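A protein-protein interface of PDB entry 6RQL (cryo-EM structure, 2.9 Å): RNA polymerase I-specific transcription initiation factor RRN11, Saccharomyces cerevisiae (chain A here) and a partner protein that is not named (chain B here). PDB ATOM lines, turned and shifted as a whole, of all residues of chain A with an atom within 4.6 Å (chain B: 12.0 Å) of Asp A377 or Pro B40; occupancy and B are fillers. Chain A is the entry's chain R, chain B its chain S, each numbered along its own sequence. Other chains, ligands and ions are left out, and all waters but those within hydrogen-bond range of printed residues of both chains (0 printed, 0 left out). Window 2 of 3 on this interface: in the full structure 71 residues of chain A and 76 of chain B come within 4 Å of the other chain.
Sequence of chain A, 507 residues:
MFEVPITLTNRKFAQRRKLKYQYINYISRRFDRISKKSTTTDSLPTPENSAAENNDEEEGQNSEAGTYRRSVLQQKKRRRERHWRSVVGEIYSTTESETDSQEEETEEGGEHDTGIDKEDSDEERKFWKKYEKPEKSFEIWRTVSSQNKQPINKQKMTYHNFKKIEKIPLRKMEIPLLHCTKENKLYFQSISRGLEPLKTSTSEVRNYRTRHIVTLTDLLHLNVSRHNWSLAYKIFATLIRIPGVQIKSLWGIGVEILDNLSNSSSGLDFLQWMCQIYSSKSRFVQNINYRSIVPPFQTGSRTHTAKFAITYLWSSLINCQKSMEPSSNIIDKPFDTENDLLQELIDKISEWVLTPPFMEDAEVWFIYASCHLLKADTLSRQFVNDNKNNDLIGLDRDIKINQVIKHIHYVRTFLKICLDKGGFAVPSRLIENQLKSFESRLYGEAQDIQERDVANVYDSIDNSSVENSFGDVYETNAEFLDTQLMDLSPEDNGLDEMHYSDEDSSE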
ATOM      1  N   LEU A 373      25.231   9.924  15.381  1.00  0.00           N
ATOM      2  CA  LEU A 373      23.826  10.170  15.081  1.00  0.00           C
ATOM      3  C   LEU A 373      23.677  11.026  13.840  1.00  0.00           C
ATOM      4  O   LEU A 373      22.858  10.720  12.970  1.00  0.00           O
ATOM      5  CB  LEU A 373      23.144  10.821  16.280  1.00  0.00           C
ATOM      6  CG  LEU A 373      21.638  11.060  16.274  1.00  0.00           C
ATOM      7  CD1 LEU A 373      21.132  10.817  17.671  1.00  0.00           C
ATOM      8  CD2 LEU A 373      21.302  12.487  15.861  1.00  0.00           C
ATOM      9  N   LEU A 374      24.468  12.091  13.734  1.00  0.00           N
ATOM     10  CA  LEU A 374      24.443  12.908  12.530  1.00  0.00           C
ATOM     11  C   LEU A 374      25.021  12.152  11.346  1.00  0.00           C
ATOM     12  O   LEU A 374      24.630  12.404  10.202  1.00  0.00           O
ATOM     13  CB  LEU A 374      25.203  14.209  12.773  1.00  0.00           C
ATOM     14  CG  LEU A 374      25.093  15.357  11.776  1.00  0.00           C
ATOM     15  CD1 LEU A 374      25.160  16.640  12.553  1.00  0.00           C
ATOM     16  CD2 LEU A 374      26.203  15.343  10.746  1.00  0.00           C
ATOM     17  N   LYS A 375      25.939  11.225  11.598  1.00  0.00           N
ATOM     18  CA  LYS A 375      26.489  10.437  10.507  1.00  0.00           C
ATOM     19  C   LYS A 375      25.480   9.417  10.005  1.00  0.00           C
ATOM     20  O   LYS A 375      25.385   9.181   8.797  1.00  0.00           O
ATOM     21  CB  LYS A 375      27.770   9.750  10.963  1.00  0.00           C
ATOM     22  CG  LYS A 375      28.542   9.104   9.848  1.00  0.00           C
ATOM     23  CD  LYS A 375      29.101  10.142   8.926  1.00  0.00           C
ATOM     24  CE  LYS A 375      29.871   9.487   7.826  1.00  0.00           C
ATOM     25  NZ  LYS A 375      31.047   8.783   8.383  1.00  0.00           N
ATOM     26  N   ALA A 376      24.707   8.823  10.912  1.00  0.00           N
ATOM     27  CA  ALA A 376      23.646   7.908  10.516  1.00  0.00           C
ATOM     28  C   ALA A 376      22.450   8.639   9.934  1.00  0.00           C
ATOM     29  O   ALA A 376      21.691   8.042   9.171  1.00  0.00           O
ATOM     30  CB  ALA A 376      23.195   7.074  11.709  1.00  0.00           C
ATOM     31  N   ASP A 377      22.258   9.904  10.300  1.00  0.00           N
ATOM     32  CA  ASP A 377      21.201  10.714   9.710  1.00  0.00           C
ATOM     33  C   ASP A 377      21.489  10.992   8.245  1.00  0.00           C
ATOM     34  O   ASP A 377      20.601  10.862   7.397  1.00  0.00           O
ATOM     35  CB  ASP A 377      21.089  12.021  10.493  1.00  0.00           C
ATOM     36  CG  ASP A 377      19.852  12.824  10.158  1.00  0.00           C
ATOM     37  OD1 ASP A 377      19.010  12.377   9.353  1.00  0.00           O
ATOM     38  OD2 ASP A 377      19.730  13.929  10.721  1.00  0.00           O
ATOM     39  N   THR A 378      22.730  11.363   7.935  1.00  0.00           N
ATOM     40  CA  THR A 378      23.089  11.793   6.590  1.00  0.00           C
ATOM     41  C   THR A 378      23.068  10.631   5.603  1.00  0.00           C
ATOM     42  O   THR A 378      22.520  10.755   4.503  1.00  0.00           O
ATOM     43  CB  THR A 378      24.463  12.451   6.622  1.00  0.00           C
ATOM     44  OG1 THR A 378      24.427  13.567   7.516  1.00  0.00           O
ATOM     45  CG2 THR A 378      24.858  12.940   5.245  1.00  0.00           C
ATOM     46  N   LEU A 379      23.629   9.488   5.984  1.00  0.00           N
ATOM     47  CA  LEU A 379      23.655   8.337   5.094  1.00  0.00           C
ATOM     48  C   LEU A 379      22.311   7.639   4.958  1.00  0.00           C
ATOM     49  O   LEU A 379      22.177   6.765   4.097  1.00  0.00           O
ATOM     50  CB  LEU A 379      24.711   7.330   5.555  1.00  0.00           C
ATOM     51  CG  LEU A 379      26.101   7.437   4.922  1.00  0.00           C
ATOM     52  CD1 LEU A 379      26.838   8.711   5.276  1.00  0.00           C
ATOM     53  CD2 LEU A 379      26.911   6.245   5.352  1.00  0.00           C
ATOM     54  N   SER A 380      21.312   8.010   5.750  1.00  0.00           N
ATOM     55  CA  SER A 380      20.002   7.374   5.664  1.00  0.00           C
ATOM     56  C   SER A 380      19.100   8.093   4.667  1.00  0.00           C
ATOM     57  O   SER A 380      18.045   8.619   5.006  1.00  0.00           O
ATOM     58  CB  SER A 380      19.364   7.320   7.041  1.00  0.00           C
ATOM     59  OG  SER A 380      18.151   6.613   7.006  1.00  0.00           O
ATOM     60  N   GLN A 434      14.496   9.102  17.303  1.00  0.00           N
ATOM     61  CA  GLN A 434      15.284   9.595  16.181  1.00  0.00           C
ATOM     62  C   GLN A 434      15.827   8.450  15.343  1.00  0.00           C
ATOM     63  O   GLN A 434      15.890   8.559  14.115  1.00  0.00           O
ATOM     64  CB  GLN A 434      16.464  10.428  16.687  1.00  0.00           C
ATOM     65  CG  GLN A 434      16.147  11.737  17.381  1.00  0.00           C
ATOM     66  CD  GLN A 434      15.703  12.818  16.428  1.00  0.00           C
ATOM     67  OE1 GLN A 434      14.551  13.243  16.444  1.00  0.00           O
ATOM     68  NE2 GLN A 434      16.623  13.277  15.588  1.00  0.00           N
ATOM     69  N   PHE A 438      15.040   6.163  11.750  1.00  0.00           N
ATOM     70  CA  PHE A 438      16.129   6.023  10.794  1.00  0.00           C
ATOM     71  C   PHE A 438      16.252   4.618  10.230  1.00  0.00           C
ATOM     72  O   PHE A 438      16.671   4.471   9.079  1.00  0.00           O
ATOM     73  CB  PHE A 438      17.462   6.415  11.429  1.00  0.00           C
ATOM     74  CG  PHE A 438      17.649   7.891  11.597  1.00  0.00           C
ATOM     75  CD1 PHE A 438      16.883   8.789  10.876  1.00  0.00           C
ATOM     76  CD2 PHE A 438      18.600   8.380  12.481  1.00  0.00           C
ATOM     77  CE1 PHE A 438      17.062  10.146  11.032  1.00  0.00           C
ATOM     78  CE2 PHE A 438      18.780   9.736  12.645  1.00  0.00           C
ATOM     79  CZ  PHE A 438      18.009  10.617  11.922  1.00  0.00           C
ATOM     80  N   ARG A 441      13.826   4.095   7.257  1.00  0.00           N
ATOM     81  CA  ARG A 441      14.393   4.438   5.960  1.00  0.00           C
ATOM     82  C   ARG A 441      15.292   3.321   5.451  1.00  0.00           C
ATOM     83  O   ARG A 441      15.442   3.147   4.238  1.00  0.00           O
ATOM     84  CB  ARG A 441      15.177   5.740   6.069  1.00  0.00           C
ATOM     85  CG  ARG A 441      14.373   6.934   6.543  1.00  0.00           C
ATOM     86  CD  ARG A 441      15.292   8.128   6.727  1.00  0.00           C
ATOM     87  NE  ARG A 441      14.630   9.300   7.287  1.00  0.00           N
ATOM     88  CZ  ARG A 441      15.270  10.414   7.628  1.00  0.00           C
ATOM     89  NH1 ARG A 441      14.606  11.442   8.131  1.00  0.00           N
ATOM     90  NH2 ARG A 441      16.578  10.495   7.468  1.00  0.00           N
ATOM     91  N   LYS B  36      22.402  20.542  21.289  1.00  0.00           N
ATOM     92  CA  LYS B  36      21.744  20.366  20.002  1.00  0.00           C
ATOM     93  C   LYS B  36      20.906  19.104  20.136  1.00  0.00           C
ATOM     94  O   LYS B  36      21.247  18.226  20.926  1.00  0.00           O
ATOM     95  CB  LYS B  36      22.740  20.242  18.832  1.00  0.00           C
ATOM     96  CG  LYS B  36      22.073  20.215  17.445  1.00  0.00           C
ATOM     97  CD  LYS B  36      23.002  20.396  16.264  1.00  0.00           C
ATOM     98  CE  LYS B  36      23.662  19.119  15.878  1.00  0.00           C
ATOM     99  NZ  LYS B  36      24.422  19.348  14.627  1.00  0.00           N
ATOM    100  N   GLN B  37      19.799  19.020  19.406  1.00  0.00           N
ATOM    101  CA  GLN B  37      19.125  17.736  19.292  1.00  0.00           C
ATOM    102  C   GLN B  37      19.294  17.061  17.941  1.00  0.00           C
ATOM    103  O   GLN B  37      19.073  15.848  17.857  1.00  0.00           O
ATOM    104  CB  GLN B  37      17.636  17.876  19.591  1.00  0.00           C
ATOM    105  CG  GLN B  37      17.364  18.013  21.055  1.00  0.00           C
ATOM    106  CD  GLN B  37      17.824  16.802  21.819  1.00  0.00           C
ATOM    107  OE1 GLN B  37      18.778  16.867  22.587  1.00  0.00           O
ATOM    108  NE2 GLN B  37      17.163  15.678  21.596  1.00  0.00           N
ATOM    109  N   GLU B  38      19.699  17.808  16.907  1.00  0.00           N
ATOM    110  CA  GLU B  38      19.750  17.337  15.520  1.00  0.00           C
ATOM    111  C   GLU B  38      18.375  16.818  15.089  1.00  0.00           C
ATOM    112  O   GLU B  38      18.092  15.620  15.077  1.00  0.00           O
ATOM    113  CB  GLU B  38      20.886  16.320  15.295  1.00  0.00           C
ATOM    114  CG  GLU B  38      21.020  15.731  13.875  1.00  0.00           C
ATOM    115  CD  GLU B  38      21.234  16.758  12.785  1.00  0.00           C
ATOM    116  OE1 GLU B  38      21.772  17.848  13.055  1.00  0.00           O
ATOM    117  OE2 GLU B  38      20.862  16.465  11.633  1.00  0.00           O
ATOM    118  N   LYS B  39      17.480  17.778  14.901  1.00  0.00           N
ATOM    119  CA  LYS B  39      16.146  17.511  14.390  1.00  0.00           C
ATOM    120  C   LYS B  39      16.125  17.654  12.877  1.00  0.00           C
ATOM    121  O   LYS B  39      15.938  18.767  12.378  1.00  0.00           O
ATOM    122  CB  LYS B  39      15.142  18.484  14.998  1.00  0.00           C
ATOM    123  CG  LYS B  39      15.013  18.419  16.499  1.00  0.00           C
ATOM    124  CD  LYS B  39      14.337  17.140  16.929  1.00  0.00           C
ATOM    125  CE  LYS B  39      14.089  17.158  18.414  1.00  0.00           C
ATOM    126  NZ  LYS B  39      13.066  18.179  18.766  1.00  0.00           N
ATOM    127  N   PRO B  40      16.245  16.567  12.113  1.00  0.00           N
ATOM    128  CA  PRO B  40      16.363  16.695  10.652  1.00  0.00           C
ATOM    129  C   PRO B  40      15.073  17.100   9.954  1.00  0.00           C
ATOM    130  O   PRO B  40      14.504  16.313   9.190  1.00  0.00           O
ATOM    131  CB  PRO B  40      16.784  15.287  10.223  1.00  0.00           C
ATOM    132  CG  PRO B  40      16.172  14.398  11.256  1.00  0.00           C
ATOM    133  CD  PRO B  40      16.212  15.158  12.543  1.00  0.00           C
ATOM    134  N   GLN B  41      14.620  18.337  10.172  1.00  0.00           N
ATOM    135  CA  GLN B  41      13.285  18.742   9.757  1.00  0.00           C
ATOM    136  C   GLN B  41      13.264  20.002   8.897  1.00  0.00           C
ATOM    137  O   GLN B  41      12.194  20.612   8.757  1.00  0.00           O
ATOM    138  CB  GLN B  41      12.382  18.942  10.983  1.00  0.00           C
ATOM    139  CG  GLN B  41      12.792  20.090  11.891  1.00  0.00           C
ATOM    140  CD  GLN B  41      11.832  20.296  13.037  1.00  0.00           C
ATOM    141  OE1 GLN B  41      10.849  19.573  13.174  1.00  0.00           O
ATOM    142  NE2 GLN B  41      12.095  21.307  13.855  1.00  0.00           N
ATOM    143  N   TRP B  42      14.409  20.401   8.325  1.00  0.00           N
ATOM    144  CA  TRP B  42      14.567  21.563   7.436  1.00  0.00           C
ATOM    145  C   TRP B  42      14.167  22.876   8.100  1.00  0.00           C
ATOM    146  O   TRP B  42      13.797  23.836   7.418  1.00  0.00           O
ATOM    147  CB  TRP B  42      13.798  21.387   6.118  1.00  0.00           C
ATOM    148  CG  TRP B  42      14.312  20.264   5.297  1.00  0.00           C
ATOM    149  CD1 TRP B  42      13.770  19.023   5.174  1.00  0.00           C
ATOM    150  CD2 TRP B  42      15.507  20.261   4.515  1.00  0.00           C
ATOM    151  NE1 TRP B  42      14.541  18.250   4.344  1.00  0.00           N
ATOM    152  CE2 TRP B  42      15.618  18.987   3.928  1.00  0.00           C
ATOM    153  CE3 TRP B  42      16.490  21.217   4.243  1.00  0.00           C
ATOM    154  CZ2 TRP B  42      16.671  18.641   3.084  1.00  0.00           C
ATOM    155  CZ3 TRP B  42      17.536  20.874   3.406  1.00  0.00           C
ATOM    156  CH2 TRP B  42      17.617  19.596   2.835  1.00  0.00           C
ATOM    157  N   LEU B  43      14.251  22.936   9.427  1.00  0.00           N
ATOM    158  CA  LEU B  43      13.723  24.040  10.209  1.00  0.00           C
ATOM    159  C   LEU B  43      14.799  24.429  11.223  1.00  0.00           C
ATOM    160  O   LEU B  43      14.568  24.474  12.426  1.00  0.00           O
ATOM    161  CB  LEU B  43      12.381  23.641  10.835  1.00  0.00           C
ATOM    162  CG  LEU B  43      11.379  24.634  11.441  1.00  0.00           C
ATOM    163  CD1 LEU B  43       9.989  24.201  11.039  1.00  0.00           C
ATOM    164  CD2 LEU B  43      11.437  24.696  12.962  1.00  0.00           C
ATOM    165  N   ARG B  44      16.022  24.657  10.709  1.00  0.00           N
ATOM    166  CA  ARG B  44      17.237  24.931  11.479  1.00  0.00           C
ATOM    167  C   ARG B  44      17.506  23.766  12.428  1.00  0.00           C
ATOM    168  O   ARG B  44      17.198  23.853  13.624  1.00  0.00           O
ATOM    169  CB  ARG B  44      17.149  26.275  12.212  1.00  0.00           C
ATOM    170  CG  ARG B  44      17.215  27.459  11.262  1.00  0.00           C
ATOM    171  CD  ARG B  44      17.263  28.789  11.989  1.00  0.00           C
ATOM    172  NE  ARG B  44      16.012  29.073  12.689  1.00  0.00           N
ATOM    173  CZ  ARG B  44      14.961  29.669  12.134  1.00  0.00           C
ATOM    174  NH1 ARG B  44      13.871  29.883  12.852  1.00  0.00           N
ATOM    175  NH2 ARG B  44      14.996  30.049  10.865  1.00  0.00           N
ATOM    176  N   PRO B  45      18.037  22.642  11.910  1.00  0.00           N
ATOM    177  CA  PRO B  45      18.049  21.374  12.657  1.00  0.00           C
ATOM    178  C   PRO B  45      18.930  21.363  13.896  1.00  0.00           C
ATOM    179  O   PRO B  45      19.916  20.625  13.964  1.00  0.00           O
ATOM    180  CB  PRO B  45      18.585  20.380  11.617  1.00  0.00           C
ATOM    181  CG  PRO B  45      19.353  21.188  10.676  1.00  0.00           C
ATOM    182  CD  PRO B  45      18.665  22.504  10.588  1.00  0.00           C
ATOM    183  N   VAL B  46      18.538  22.153  14.891  1.00  0.00           N
ATOM    184  CA  VAL B  46      19.356  22.462  16.054  1.00  0.00           C
ATOM    185  C   VAL B  46      18.439  23.128  17.070  1.00  0.00           C
ATOM    186  O   VAL B  46      17.518  23.859  16.701  1.00  0.00           O
ATOM    187  CB  VAL B  46      20.568  23.344  15.640  1.00  0.00           C
ATOM    188  CG1 VAL B  46      20.121  24.628  14.958  1.00  0.00           C
ATOM    189  CG2 VAL B  46      21.463  23.691  16.796  1.00  0.00           C
ATOM    190  N   ASP B  47      18.647  22.834  18.349  1.00  0.00           N
ATOM    191  CA  ASP B  47      18.001  23.668  19.350  1.00  0.00           C
ATOM    192  C   ASP B  47      19.058  24.318  20.235  1.00  0.00           C
ATOM    193  O   ASP B  47      19.033  24.195  21.458  1.00  0.00           O
ATOM    194  CB  ASP B  47      16.934  22.911  20.142  1.00  0.00           C
ATOM    195  CG  ASP B  47      17.452  21.691  20.822  1.00  0.00           C
ATOM    196  OD1 ASP B  47      18.614  21.309  20.575  1.00  0.00           O
ATOM    197  OD2 ASP B  47      16.683  21.137  21.640  1.00  0.00           O
ATOM    198  N   ASP B  48      20.036  24.919  19.566  1.00  0.00           N
ATOM    199  CA  ASP B  48      20.884  26.002  20.045  1.00  0.00           C
ATOM    200  C   ASP B  48      20.127  26.905  21.014  1.00  0.00           C
ATOM    201  O   ASP B  48      19.035  27.388  20.707  1.00  0.00           O
ATOM    202  CB  ASP B  48      21.328  26.771  18.781  1.00  0.00           C
ATOM    203  CG  ASP B  48      22.327  27.895  19.018  1.00  0.00           C
ATOM    204  OD1 ASP B  48      22.678  28.241  20.154  1.00  0.00           O
ATOM    205  OD2 ASP B  48      22.771  28.461  17.995  1.00  0.00           O
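Leu A373 touches Glu B38 (CD2 to CG, 3.8 Å).
NZ of Lys B36 touches CD1 of Leu A374, at 3.5 Å.
Glu B38 touches Leu A374.
Asp A377 touches Pro B40 (OD2 to CB, 3.3 Å).
Gln A434 touches Lys B39.
Gln A434 touches Pro B40.
Printed residues of chain B that touch a printed residue of chain A: Lys B36, Glu B38, Lys B39 and Pro B40.
Hydrophobic or aromatic side chains of chain B within 4 Å of the printed part of chain A: Pro B40.
Printed residues of chain A that touch a printed residue of chain B: Leu A373, Leu A374, Asp A377 and Gln A434.
Hydrophobic or aromatic side chains of chain A within 4 Å of the printed part of chain B: Leu A373 and Leu A374.
Among the printed residues, 8 pairs touch across the chains.
Among the printed residues, no Asp or Glu carboxylate lies within 4 Å of a Lys or Arg side-chain nitrogen of the other chain.
Of the printed residues of chain B, Asp A377 touches Glu B38 (2.9 Å) and Pro B40 (3.3 Å).
Of the printed residues of chain B, Leu A373 touches Glu B38.
Leu A374 touches just these residues of chain B: Lys B36 (3.5 Å) and Glu B38 (3.6 Å).
No residue of chain B comes within 4 Å of Ala A376.
No residue of chain B comes within 4 Å of Thr A378.
No residue of chain B comes within 4 Å of Leu A379.
No residue of chain B comes within 4 Å of Ser A380.
Printed residues of chain A within 4 Å of Lys B36: Leu A374 (3.5 Å).
Printed residues of chain A within 4 Å of Lys B39: Gln A434.
Printed residues of chain A within 4 Å of Glu B38: Leu A373 (3.8 Å), Leu A374 (3.6 Å), Asp A377 (2.9 Å) and Gln A434 (2.8 Å).
The nearest residue of chain B that does not touch Asp A377 is Lys B39 (5.6 Å).
The side-chain hydroxyl of Thr A378 is in hydrogen-bond range of the backbone carbonyl oxygen of Leu A374 (2.9 Å).
The guanidinium group of Arg A441 is in salt-bridge range of the side-chain carboxylate of Asp A377, 3.6 Å away.
The side-chain carboxylate of Glu B38 is in salt-bridge range of the side-chain amino group of Lys B36 (3.4 Å).
The side-chain carboxylate of Glu B38 lies close to the side-chain carboxylate of Asp A377, 2.9 Å away.
The backbone carbonyl oxygen of Glu B38 sits at hydrogen-bond distance from the side-chain amide nitrogen of Gln A434 (2.8 Å).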
